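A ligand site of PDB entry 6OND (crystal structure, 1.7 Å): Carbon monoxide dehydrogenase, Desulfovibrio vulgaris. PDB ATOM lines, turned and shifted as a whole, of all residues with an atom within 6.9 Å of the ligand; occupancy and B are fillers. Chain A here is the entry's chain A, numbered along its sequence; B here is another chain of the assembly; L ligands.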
ATOM      1  N   THR A  58     -10.609  -3.166  -6.527  1.00  0.00           N
ATOM      2  CA  THR A  58     -10.197  -1.864  -7.020  1.00  0.00           C
ATOM      3  C   THR A  58     -11.215  -0.835  -6.556  1.00  0.00           C
ATOM      4  O   THR A  58     -12.403  -1.125  -6.442  1.00  0.00           O
ATOM      5  CB  THR A  58     -10.100  -1.902  -8.568  1.00  0.00           C
ATOM      6  OG1 THR A  58      -9.821  -0.592  -9.081  1.00  0.00           O
ATOM      7  CG2 THR A  58     -11.386  -2.440  -9.181  1.00  0.00           C
ATOM      8  N   CYS A  59     -10.740   0.382  -6.266  1.00  0.00           N
ATOM      9  CA  CYS A  59     -11.614   1.423  -5.742  1.00  0.00           C
ATOM     10  C   CYS A  59     -11.281   2.742  -6.412  1.00  0.00           C
ATOM     11  O   CYS A  59     -10.113   3.103  -6.550  1.00  0.00           O
ATOM     12  CB  CYS A  59     -11.415   1.540  -4.221  1.00  0.00           C
ATOM     13  SG  CYS A  59     -12.587   2.692  -3.429  1.00  0.00           S
ATOM     14  N   ARG A  60     -12.318   3.475  -6.846  1.00  0.00           N
ATOM     15  CA  ARG A  60     -12.159   4.802  -7.425  1.00  0.00           C
ATOM     16  C   ARG A  60     -13.064   5.796  -6.723  1.00  0.00           C
ATOM     17  O   ARG A  60     -13.578   6.717  -7.343  1.00  0.00           O
ATOM     18  CB  ARG A  60     -12.458   4.793  -8.924  1.00  0.00           C
ATOM     19  CG  ARG A  60     -11.740   3.697  -9.694  1.00  0.00           C
ATOM     20  CD  ARG A  60     -12.325   3.562 -11.100  1.00  0.00           C
ATOM     21  NE  ARG A  60     -13.618   2.883 -11.115  1.00  0.00           N
ATOM     22  CZ  ARG A  60     -14.576   3.134 -12.005  1.00  0.00           C
ATOM     23  NH1 ARG A  60     -14.386   4.061 -12.926  1.00  0.00           N
ATOM     24  NH2 ARG A  60     -15.718   2.462 -11.966  1.00  0.00           N
ATOM     25  N   ASN A  61     -13.288   5.612  -5.424  1.00  0.00           N
ATOM     26  CA  ASN A  61     -14.280   6.423  -4.722  1.00  0.00           C
ATOM     27  C   ASN A  61     -13.743   7.763  -4.255  1.00  0.00           C
ATOM     28  O   ASN A  61     -14.525   8.556  -3.716  1.00  0.00           O
ATOM     29  CB  ASN A  61     -14.899   5.649  -3.556  1.00  0.00           C
ATOM     30  CG  ASN A  61     -15.843   4.554  -4.023  1.00  0.00           C
ATOM     31  OD1 ASN A  61     -15.888   4.251  -5.212  1.00  0.00           O
ATOM     32  ND2 ASN A  61     -16.571   3.943  -3.093  1.00  0.00           N
ATOM     33  N   CYS A  62     -12.450   8.043  -4.421  1.00  0.00           N
ATOM     34  CA  CYS A  62     -11.906   9.365  -4.154  1.00  0.00           C
ATOM     35  C   CYS A  62     -10.626   9.512  -4.961  1.00  0.00           C
ATOM     36  O   CYS A  62     -10.150   8.553  -5.571  1.00  0.00           O
ATOM     37  CB  CYS A  62     -11.645   9.599  -2.654  1.00  0.00           C
ATOM     38  SG  CYS A  62     -10.124   8.827  -1.973  1.00  0.00           S
ATOM     39  N   ILE A  63     -10.087  10.728  -4.992  1.00  0.00           N
ATOM     40  CA  ILE A  63      -8.880  10.972  -5.769  1.00  0.00           C
ATOM     41  C   ILE A  63      -7.625  10.989  -4.897  1.00  0.00           C
ATOM     42  O   ILE A  63      -6.565  11.415  -5.363  1.00  0.00           O
ATOM     43  CB  ILE A  63      -8.961  12.171  -6.729  1.00  0.00           C
ATOM     44  CG1 ILE A  63      -9.032  13.488  -5.945  1.00  0.00           C
ATOM     45  CG2 ILE A  63     -10.155  11.984  -7.704  1.00  0.00           C
ATOM     46  CD1 ILE A  63      -8.346  14.689  -6.673  1.00  0.00           C
ATOM     47  N   MET A  64      -7.705  10.515  -3.647  1.00  0.00           N
ATOM     48  CA  MET A  64      -6.490   9.970  -3.055  1.00  0.00           C
ATOM     49  C   MET A  64      -6.067   8.717  -3.813  1.00  0.00           C
ATOM     50  O   MET A  64      -4.872   8.430  -3.928  1.00  0.00           O
ATOM     51  CB  MET A  64      -6.661   9.662  -1.570  1.00  0.00           C
ATOM     52  CG  MET A  64      -6.956  10.884  -0.706  1.00  0.00           C
ATOM     53  SD  MET A  64      -6.449  10.614   1.010  1.00  0.00           S
ATOM     54  CE  MET A  64      -7.446   9.198   1.473  1.00  0.00           C
ATOM     55  N   GLY A  65      -7.052   7.981  -4.330  1.00  0.00           N
ATOM     56  CA  GLY A  65      -6.840   6.853  -5.211  1.00  0.00           C
ATOM     57  C   GLY A  65      -6.634   7.294  -6.655  1.00  0.00           C
ATOM     58  O   GLY A  65      -6.239   8.429  -6.933  1.00  0.00           O
ATOM     59  N   PRO A  66      -6.936   6.403  -7.602  1.00  0.00           N
ATOM     60  CA  PRO A  66      -7.562   5.092  -7.434  1.00  0.00           C
ATOM     61  C   PRO A  66      -6.627   4.044  -6.847  1.00  0.00           C
ATOM     62  O   PRO A  66      -5.395   4.159  -6.973  1.00  0.00           O
ATOM     63  CB  PRO A  66      -7.973   4.712  -8.862  1.00  0.00           C
ATOM     64  CG  PRO A  66      -7.003   5.451  -9.744  1.00  0.00           C
ATOM     65  CD  PRO A  66      -6.726   6.750  -9.026  1.00  0.00           C
ATOM     66  N   CYS A  67      -7.207   3.046  -6.202  1.00  0.00           N
ATOM     67  CA  CYS A  67      -6.463   2.041  -5.463  1.00  0.00           C
ATOM     68  C   CYS A  67      -6.777   0.646  -5.992  1.00  0.00           C
ATOM     69  O   CYS A  67      -7.891   0.379  -6.463  1.00  0.00           O
ATOM     70  CB  CYS A  67      -6.823   2.098  -3.975  1.00  0.00           C
ATOM     71  SG  CYS A  67      -6.509   3.724  -3.195  1.00  0.00           S
ATOM     72  N   ARG A  68      -5.789  -0.245  -5.878  1.00  0.00           N
ATOM     73  CA  ARG A  68      -5.969  -1.659  -6.153  1.00  0.00           C
ATOM     74  C   ARG A  68      -5.412  -2.452  -4.976  1.00  0.00           C
ATOM     75  O   ARG A  68      -4.401  -2.075  -4.394  1.00  0.00           O
ATOM     76  CB  ARG A  68      -5.215  -2.063  -7.414  1.00  0.00           C
ATOM     77  CG  ARG A  68      -5.902  -1.601  -8.705  1.00  0.00           C
ATOM     78  CD  ARG A  68      -4.957  -1.603  -9.895  1.00  0.00           C
ATOM     79  NE  ARG A  68      -3.850  -0.678  -9.672  1.00  0.00           N
ATOM     80  CZ  ARG A  68      -2.729  -0.666 -10.372  1.00  0.00           C
ATOM     81  NH1 ARG A  68      -2.570  -1.508 -11.376  1.00  0.00           N
ATOM     82  NH2 ARG A  68      -1.765   0.196 -10.073  1.00  0.00           N
ATOM     83  N   ILE A  69      -6.054  -3.559  -4.631  1.00  0.00           N
ATOM     84  CA  ILE A  69      -5.579  -4.411  -3.540  1.00  0.00           C
ATOM     85  C   ILE A  69      -4.940  -5.645  -4.165  1.00  0.00           C
ATOM     86  O   ILE A  69      -5.593  -6.385  -4.911  1.00  0.00           O
ATOM     87  CB  ILE A  69      -6.705  -4.791  -2.569  1.00  0.00           C
ATOM     88  CG1 ILE A  69      -7.357  -3.529  -2.001  1.00  0.00           C
ATOM     89  CG2 ILE A  69      -6.165  -5.683  -1.451  1.00  0.00           C
ATOM     90  CD1 ILE A  69      -6.368  -2.521  -1.368  1.00  0.00           C
ATOM     91  N   LEU A  79      -3.577  -2.335   1.313  1.00  0.00           N
ATOM     92  CA  LEU A  79      -4.612  -1.405   1.718  1.00  0.00           C
ATOM     93  C   LEU A  79      -4.686  -0.248   0.725  1.00  0.00           C
ATOM     94  O   LEU A  79      -3.697   0.113   0.081  1.00  0.00           O
ATOM     95  CB  LEU A  79      -4.296  -0.801   3.088  1.00  0.00           C
ATOM     96  CG  LEU A  79      -4.060  -1.800   4.222  1.00  0.00           C
ATOM     97  CD1 LEU A  79      -3.558  -1.038   5.449  1.00  0.00           C
ATOM     98  CD2 LEU A  79      -5.347  -2.563   4.538  1.00  0.00           C
ATOM     99  N   GLY A  80      -5.868   0.344   0.645  1.00  0.00           N
ATOM    100  CA  GLY A  80      -6.021   1.598  -0.067  1.00  0.00           C
ATOM    101  C   GLY A  80      -5.336   2.746   0.656  1.00  0.00           C
ATOM    102  O   GLY A  80      -4.859   2.623   1.793  1.00  0.00           O
ATOM    103  N   VAL A  81      -5.289   3.899  -0.019  1.00  0.00           N
ATOM    104  CA  VAL A  81      -4.614   5.065   0.546  1.00  0.00           C
ATOM    105  C   VAL A  81      -5.250   5.492   1.859  1.00  0.00           C
ATOM    106  O   VAL A  81      -4.569   5.898   2.801  1.00  0.00           O
ATOM    107  CB  VAL A  81      -4.549   6.203  -0.485  1.00  0.00           C
ATOM    108  CG1 VAL A  81      -3.910   7.443   0.142  1.00  0.00           C
ATOM    109  CG2 VAL A  81      -3.741   5.752  -1.692  1.00  0.00           C
ATOM    110  N   CYS A  82      -6.577   5.387   1.957  1.00  0.00           N
ATOM    111  CA  CYS A  82      -7.266   5.705   3.206  1.00  0.00           C
ATOM    112  C   CYS A  82      -7.108   4.624   4.275  1.00  0.00           C
ATOM    113  O   CYS A  82      -7.557   4.843   5.408  1.00  0.00           O
ATOM    114  CB  CYS A  82      -8.760   5.921   2.944  1.00  0.00           C
ATOM    115  SG  CYS A  82      -9.621   4.412   2.291  1.00  0.00           S
ATOM    116  N   GLY A  83      -6.516   3.471   3.951  1.00  0.00           N
ATOM    117  CA  GLY A  83      -6.388   2.366   4.886  1.00  0.00           C
ATOM    118  C   GLY A  83      -7.394   1.252   4.702  1.00  0.00           C
ATOM    119  O   GLY A  83      -7.351   0.272   5.464  1.00  0.00           O
ATOM    120  N   ALA A  84      -8.306   1.364   3.739  1.00  0.00           N
ATOM    121  CA  ALA A  84      -9.361   0.373   3.579  1.00  0.00           C
ATOM    122  C   ALA A  84      -8.784  -0.917   3.023  1.00  0.00           C
ATOM    123  O   ALA A  84      -7.900  -0.894   2.155  1.00  0.00           O
ATOM    124  CB  ALA A  84     -10.462   0.903   2.655  1.00  0.00           C
ATOM    125  N   ASP A  85      -9.268  -2.051   3.530  1.00  0.00           N
ATOM    126  CA  ASP A  85      -8.799  -3.351   3.094  1.00  0.00           C
ATOM    127  C   ASP A  85      -9.726  -3.948   2.032  1.00  0.00           C
ATOM    128  O   ASP A  85     -10.717  -3.334   1.603  1.00  0.00           O
ATOM    129  CB  ASP A  85      -8.549  -4.284   4.290  1.00  0.00           C
ATOM    130  CG  ASP A  85      -9.806  -4.637   5.043  1.00  0.00           C
ATOM    131  OD1 ASP A  85     -10.909  -4.295   4.572  1.00  0.00           O
ATOM    132  OD2 ASP A  85      -9.703  -5.259   6.136  1.00  0.00           O
ATOM    133  N   ILE A  89     -13.435  -2.661   0.564  1.00  0.00           N
ATOM    134  CA  ILE A  89     -13.492  -2.223  -0.829  1.00  0.00           C
ATOM    135  C   ILE A  89     -14.464  -3.073  -1.631  1.00  0.00           C
ATOM    136  O   ILE A  89     -15.292  -2.562  -2.390  1.00  0.00           O
ATOM    137  CB  ILE A  89     -12.086  -2.197  -1.447  1.00  0.00           C
ATOM    138  CG1 ILE A  89     -11.295  -1.015  -0.884  1.00  0.00           C
ATOM    139  CG2 ILE A  89     -12.151  -2.116  -2.990  1.00  0.00           C
ATOM    140  CD1 ILE A  89      -9.807  -1.084  -1.151  1.00  0.00           C
ATOM    141  N   ARG A  92     -18.128  -2.387  -0.374  1.00  0.00           N
ATOM    142  CA  ARG A  92     -18.633  -1.107  -0.862  1.00  0.00           C
ATOM    143  C   ARG A  92     -18.958  -1.169  -2.357  1.00  0.00           C
ATOM    144  O   ARG A  92     -19.968  -0.611  -2.789  1.00  0.00           O
ATOM    145  CB  ARG A  92     -17.620   0.008  -0.612  1.00  0.00           C
ATOM    146  CG  ARG A  92     -17.477   0.391   0.854  1.00  0.00           C
ATOM    147  CD  ARG A  92     -16.654   1.686   1.023  1.00  0.00           C
ATOM    148  NE  ARG A  92     -15.347   1.595   0.375  1.00  0.00           N
ATOM    149  CZ  ARG A  92     -14.284   2.313   0.753  1.00  0.00           C
ATOM    150  NH1 ARG A  92     -14.384   3.133   1.797  1.00  0.00           N
ATOM    151  NH2 ARG A  92     -13.122   2.193   0.097  1.00  0.00           N
ATOM    152  N   THR A 209     -20.855   4.384   1.379  1.00  0.00           N
ATOM    153  CA  THR A 209     -19.742   3.919   0.564  1.00  0.00           C
ATOM    154  C   THR A 209     -18.741   5.025   0.209  1.00  0.00           C
ATOM    155  O   THR A 209     -17.732   4.730  -0.431  1.00  0.00           O
ATOM    156  CB  THR A 209     -20.245   3.204  -0.682  1.00  0.00           C
ATOM    157  OG1 THR A 209     -21.169   4.052  -1.400  1.00  0.00           O
ATOM    158  CG2 THR A 209     -20.952   1.892  -0.307  1.00  0.00           C
ATOM    159  N   HIS A 210     -18.998   6.280   0.619  1.00  0.00           N
ATOM    160  CA  HIS A 210     -18.011   7.350   0.551  1.00  0.00           C
ATOM    161  C   HIS A 210     -16.811   7.003   1.436  1.00  0.00           C
ATOM    162  O   HIS A 210     -16.941   6.297   2.440  1.00  0.00           O
ATOM    163  CB  HIS A 210     -18.691   8.640   1.077  1.00  0.00           C
ATOM    164  CG  HIS A 210     -17.907   9.902   0.865  1.00  0.00           C
ATOM    165  ND1 HIS A 210     -16.842  10.257   1.649  1.00  0.00           N
ATOM    166  CD2 HIS A 210     -18.091  10.931  -0.015  1.00  0.00           C
ATOM    167  CE1 HIS A 210     -16.360  11.415   1.249  1.00  0.00           C
ATOM    168  NE2 HIS A 210     -17.095  11.857   0.242  1.00  0.00           N
ATOM    169  N   MET A 211     -15.625   7.524   1.072  1.00  0.00           N
ATOM    170  CA  MET A 211     -14.431   7.286   1.903  1.00  0.00           C
ATOM    171  C   MET A 211     -14.721   7.612   3.358  1.00  0.00           C
ATOM    172  O   MET A 211     -15.322   8.644   3.669  1.00  0.00           O
ATOM    173  CB  MET A 211     -13.259   8.166   1.434  1.00  0.00           C
ATOM    174  CG  MET A 211     -11.889   7.810   2.058  1.00  0.00           C
ATOM    175  SD  MET A 211     -11.617   8.249   3.826  1.00  0.00           S
ATOM    176  CE  MET A 211     -10.536   9.680   3.708  1.00  0.00           C
ATOM    177  N   GLY A 212     -14.283   6.744   4.261  1.00  0.00           N
ATOM    178  CA  GLY A 212     -14.337   7.091   5.671  1.00  0.00           C
ATOM    179  C   GLY A 212     -15.709   7.128   6.287  1.00  0.00           C
ATOM    180  O   GLY A 212     -15.916   7.829   7.294  1.00  0.00           O
ATOM    181  N   GLN B  46       0.475   2.985  -3.779  1.00  0.00           N
ATOM    182  CA  GLN B  46      -0.544   2.979  -4.837  1.00  0.00           C
ATOM    183  C   GLN B  46      -0.130   3.784  -6.065  1.00  0.00           C
ATOM    184  O   GLN B  46      -0.975   4.056  -6.927  1.00  0.00           O
ATOM    185  CB  GLN B  46      -1.889   3.458  -4.311  1.00  0.00           C
ATOM    186  CG  GLN B  46      -2.546   2.539  -3.293  1.00  0.00           C
ATOM    187  CD  GLN B  46      -3.064   1.246  -3.899  1.00  0.00           C
ATOM    188  OE1 GLN B  46      -3.252   1.143  -5.119  1.00  0.00           O
ATOM    189  NE2 GLN B  46      -3.296   0.240  -3.050  1.00  0.00           N
ATOM    190  N   PRO B 351      -9.994   4.595   7.936  1.00  0.00           N
ATOM    191  CA  PRO B 351      -9.934   3.378   8.752  1.00  0.00           C
ATOM    192  C   PRO B 351      -8.556   3.077   9.289  1.00  0.00           C
ATOM    193  O   PRO B 351      -8.438   2.296  10.245  1.00  0.00           O
ATOM    194  CB  PRO B 351     -10.432   2.283   7.800  1.00  0.00           C
ATOM    195  CG  PRO B 351     -10.246   2.836   6.431  1.00  0.00           C
ATOM    196  CD  PRO B 351     -10.487   4.330   6.569  1.00  0.00           C
ATOM    197  N   TYR B 561      -9.891  15.964  -2.288  1.00  0.00           N
ATOM    198  CA  TYR B 561      -9.851  14.527  -2.503  1.00  0.00           C
ATOM    199  C   TYR B 561     -11.225  13.868  -2.608  1.00  0.00           C
ATOM    200  O   TYR B 561     -11.340  12.882  -3.321  1.00  0.00           O
ATOM    201  CB  TYR B 561      -9.021  13.813  -1.403  1.00  0.00           C
ATOM    202  CG  TYR B 561      -9.906  13.283  -0.284  1.00  0.00           C
ATOM    203  CD1 TYR B 561     -10.512  12.033  -0.376  1.00  0.00           C
ATOM    204  CD2 TYR B 561     -10.196  14.064   0.827  1.00  0.00           C
ATOM    205  CE1 TYR B 561     -11.366  11.588   0.592  1.00  0.00           C
ATOM    206  CE2 TYR B 561     -11.050  13.626   1.807  1.00  0.00           C
ATOM    207  CZ  TYR B 561     -11.632  12.381   1.689  1.00  0.00           C
ATOM    208  OH  TYR B 561     -12.494  11.916   2.660  1.00  0.00           O
HETATM  209 FE1  LIG L   1     -11.130   4.043  -2.359  1.00  0.00          FE
HETATM  210 FE2  LIG L   1      -8.480   4.476  -2.341  1.00  0.00          FE
HETATM  211 FE3  LIG L   1      -9.891   4.656   0.028  1.00  0.00          FE
HETATM  212 FE4  LIG L   1     -10.218   6.554  -1.965  1.00  0.00          FE
HETATM  213  S1  LIG L   1      -8.295   6.115  -0.780  1.00  0.00           S
HETATM  214  S2  LIG L   1     -11.882   5.501  -0.795  1.00  0.00           S
HETATM  215  S3  LIG L   1      -9.973   5.325  -3.858  1.00  0.00           S
HETATM  216  S4  LIG L   1      -9.572   2.781  -1.240  1.00  0.00           S
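The backbone carbonyl oxygen (O) of Cys 67 sits at hydrogen-bond distance from the backbone NH (N) of Cys 59 (2.9 Å).
SG of Cys 59 lies close to NH2 of Arg 92 (3.6 Å).
SG of Cys 59 lies close to N of Asn 61, 3.6 Å away.
N of Met 64 lies close to SG of Cys 62, 3.4 Å away.
The side-chain sulfur (SG) of Cys 67 sits close to the backbone NH (N) of Val 81 (3.4 Å).
The side-chain hydroxyl (OG1) of Thr 58 sits close to the backbone carbonyl oxygen (O) of Cys 67 (3.4 Å).
The side-chain sulfur (SG) of Cys 82 sits close to the backbone NH (N) of Ala 84.
The backbone carbonyl oxygen (O) of Thr 209 is in hydrogen-bond range of the side-chain amide nitrogen (ND2) of Asn 61, at 3.0 Å.
The side-chain sulfur (SG) of Cys 59 binds an iron atom (FE1) of the ligand (2.3 Å).
N of Cys 62 sits close to S3 of the ligand, at 3.7 Å.
An iron atom (FE4) of the ligand is bound by the side-chain sulfur of Cys 62 (2.3 Å).
The side-chain sulfur (SG) of Cys 67 is bound to an iron atom (FE2) of the ligand.
The backbone NH (N) of Cys 82 lies close to a sulfur (S1) of the ligand (3.3 Å).
The side-chain sulfur (SG) of Cys 82 is bound to an iron atom (FE3) of the ligand (2.3 Å).
S2 of the ligand sits close to NH2 of Arg 92 (3.6 Å).
A sulfur (S3) of the ligand lies close to the backbone NH (N) of Asn 61 (3.7 Å).
Residues that only touch the ligand: Met 211 (3.7 Å), Gly 65 (3.7 Å), Val 81 (3.8 Å), Ile 89 (3.9 Å), Met 64 (3.9 Å) and Gly 80 (3.9 Å).
Hydrophobic or aromatic side chains that line the ligand: Met 64, Val 81, Ile 89 and Met 211.
Within 4 Å of the ligand: Cys 59, Asn 61, Cys 62, Met 64, Gly 65, Cys 67, Gly 80, Val 81, Cys 82, Ile 89, Arg 92 and Met 211.
Along chain A the residues within 4 Å of the ligand span positions 59 to 211.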
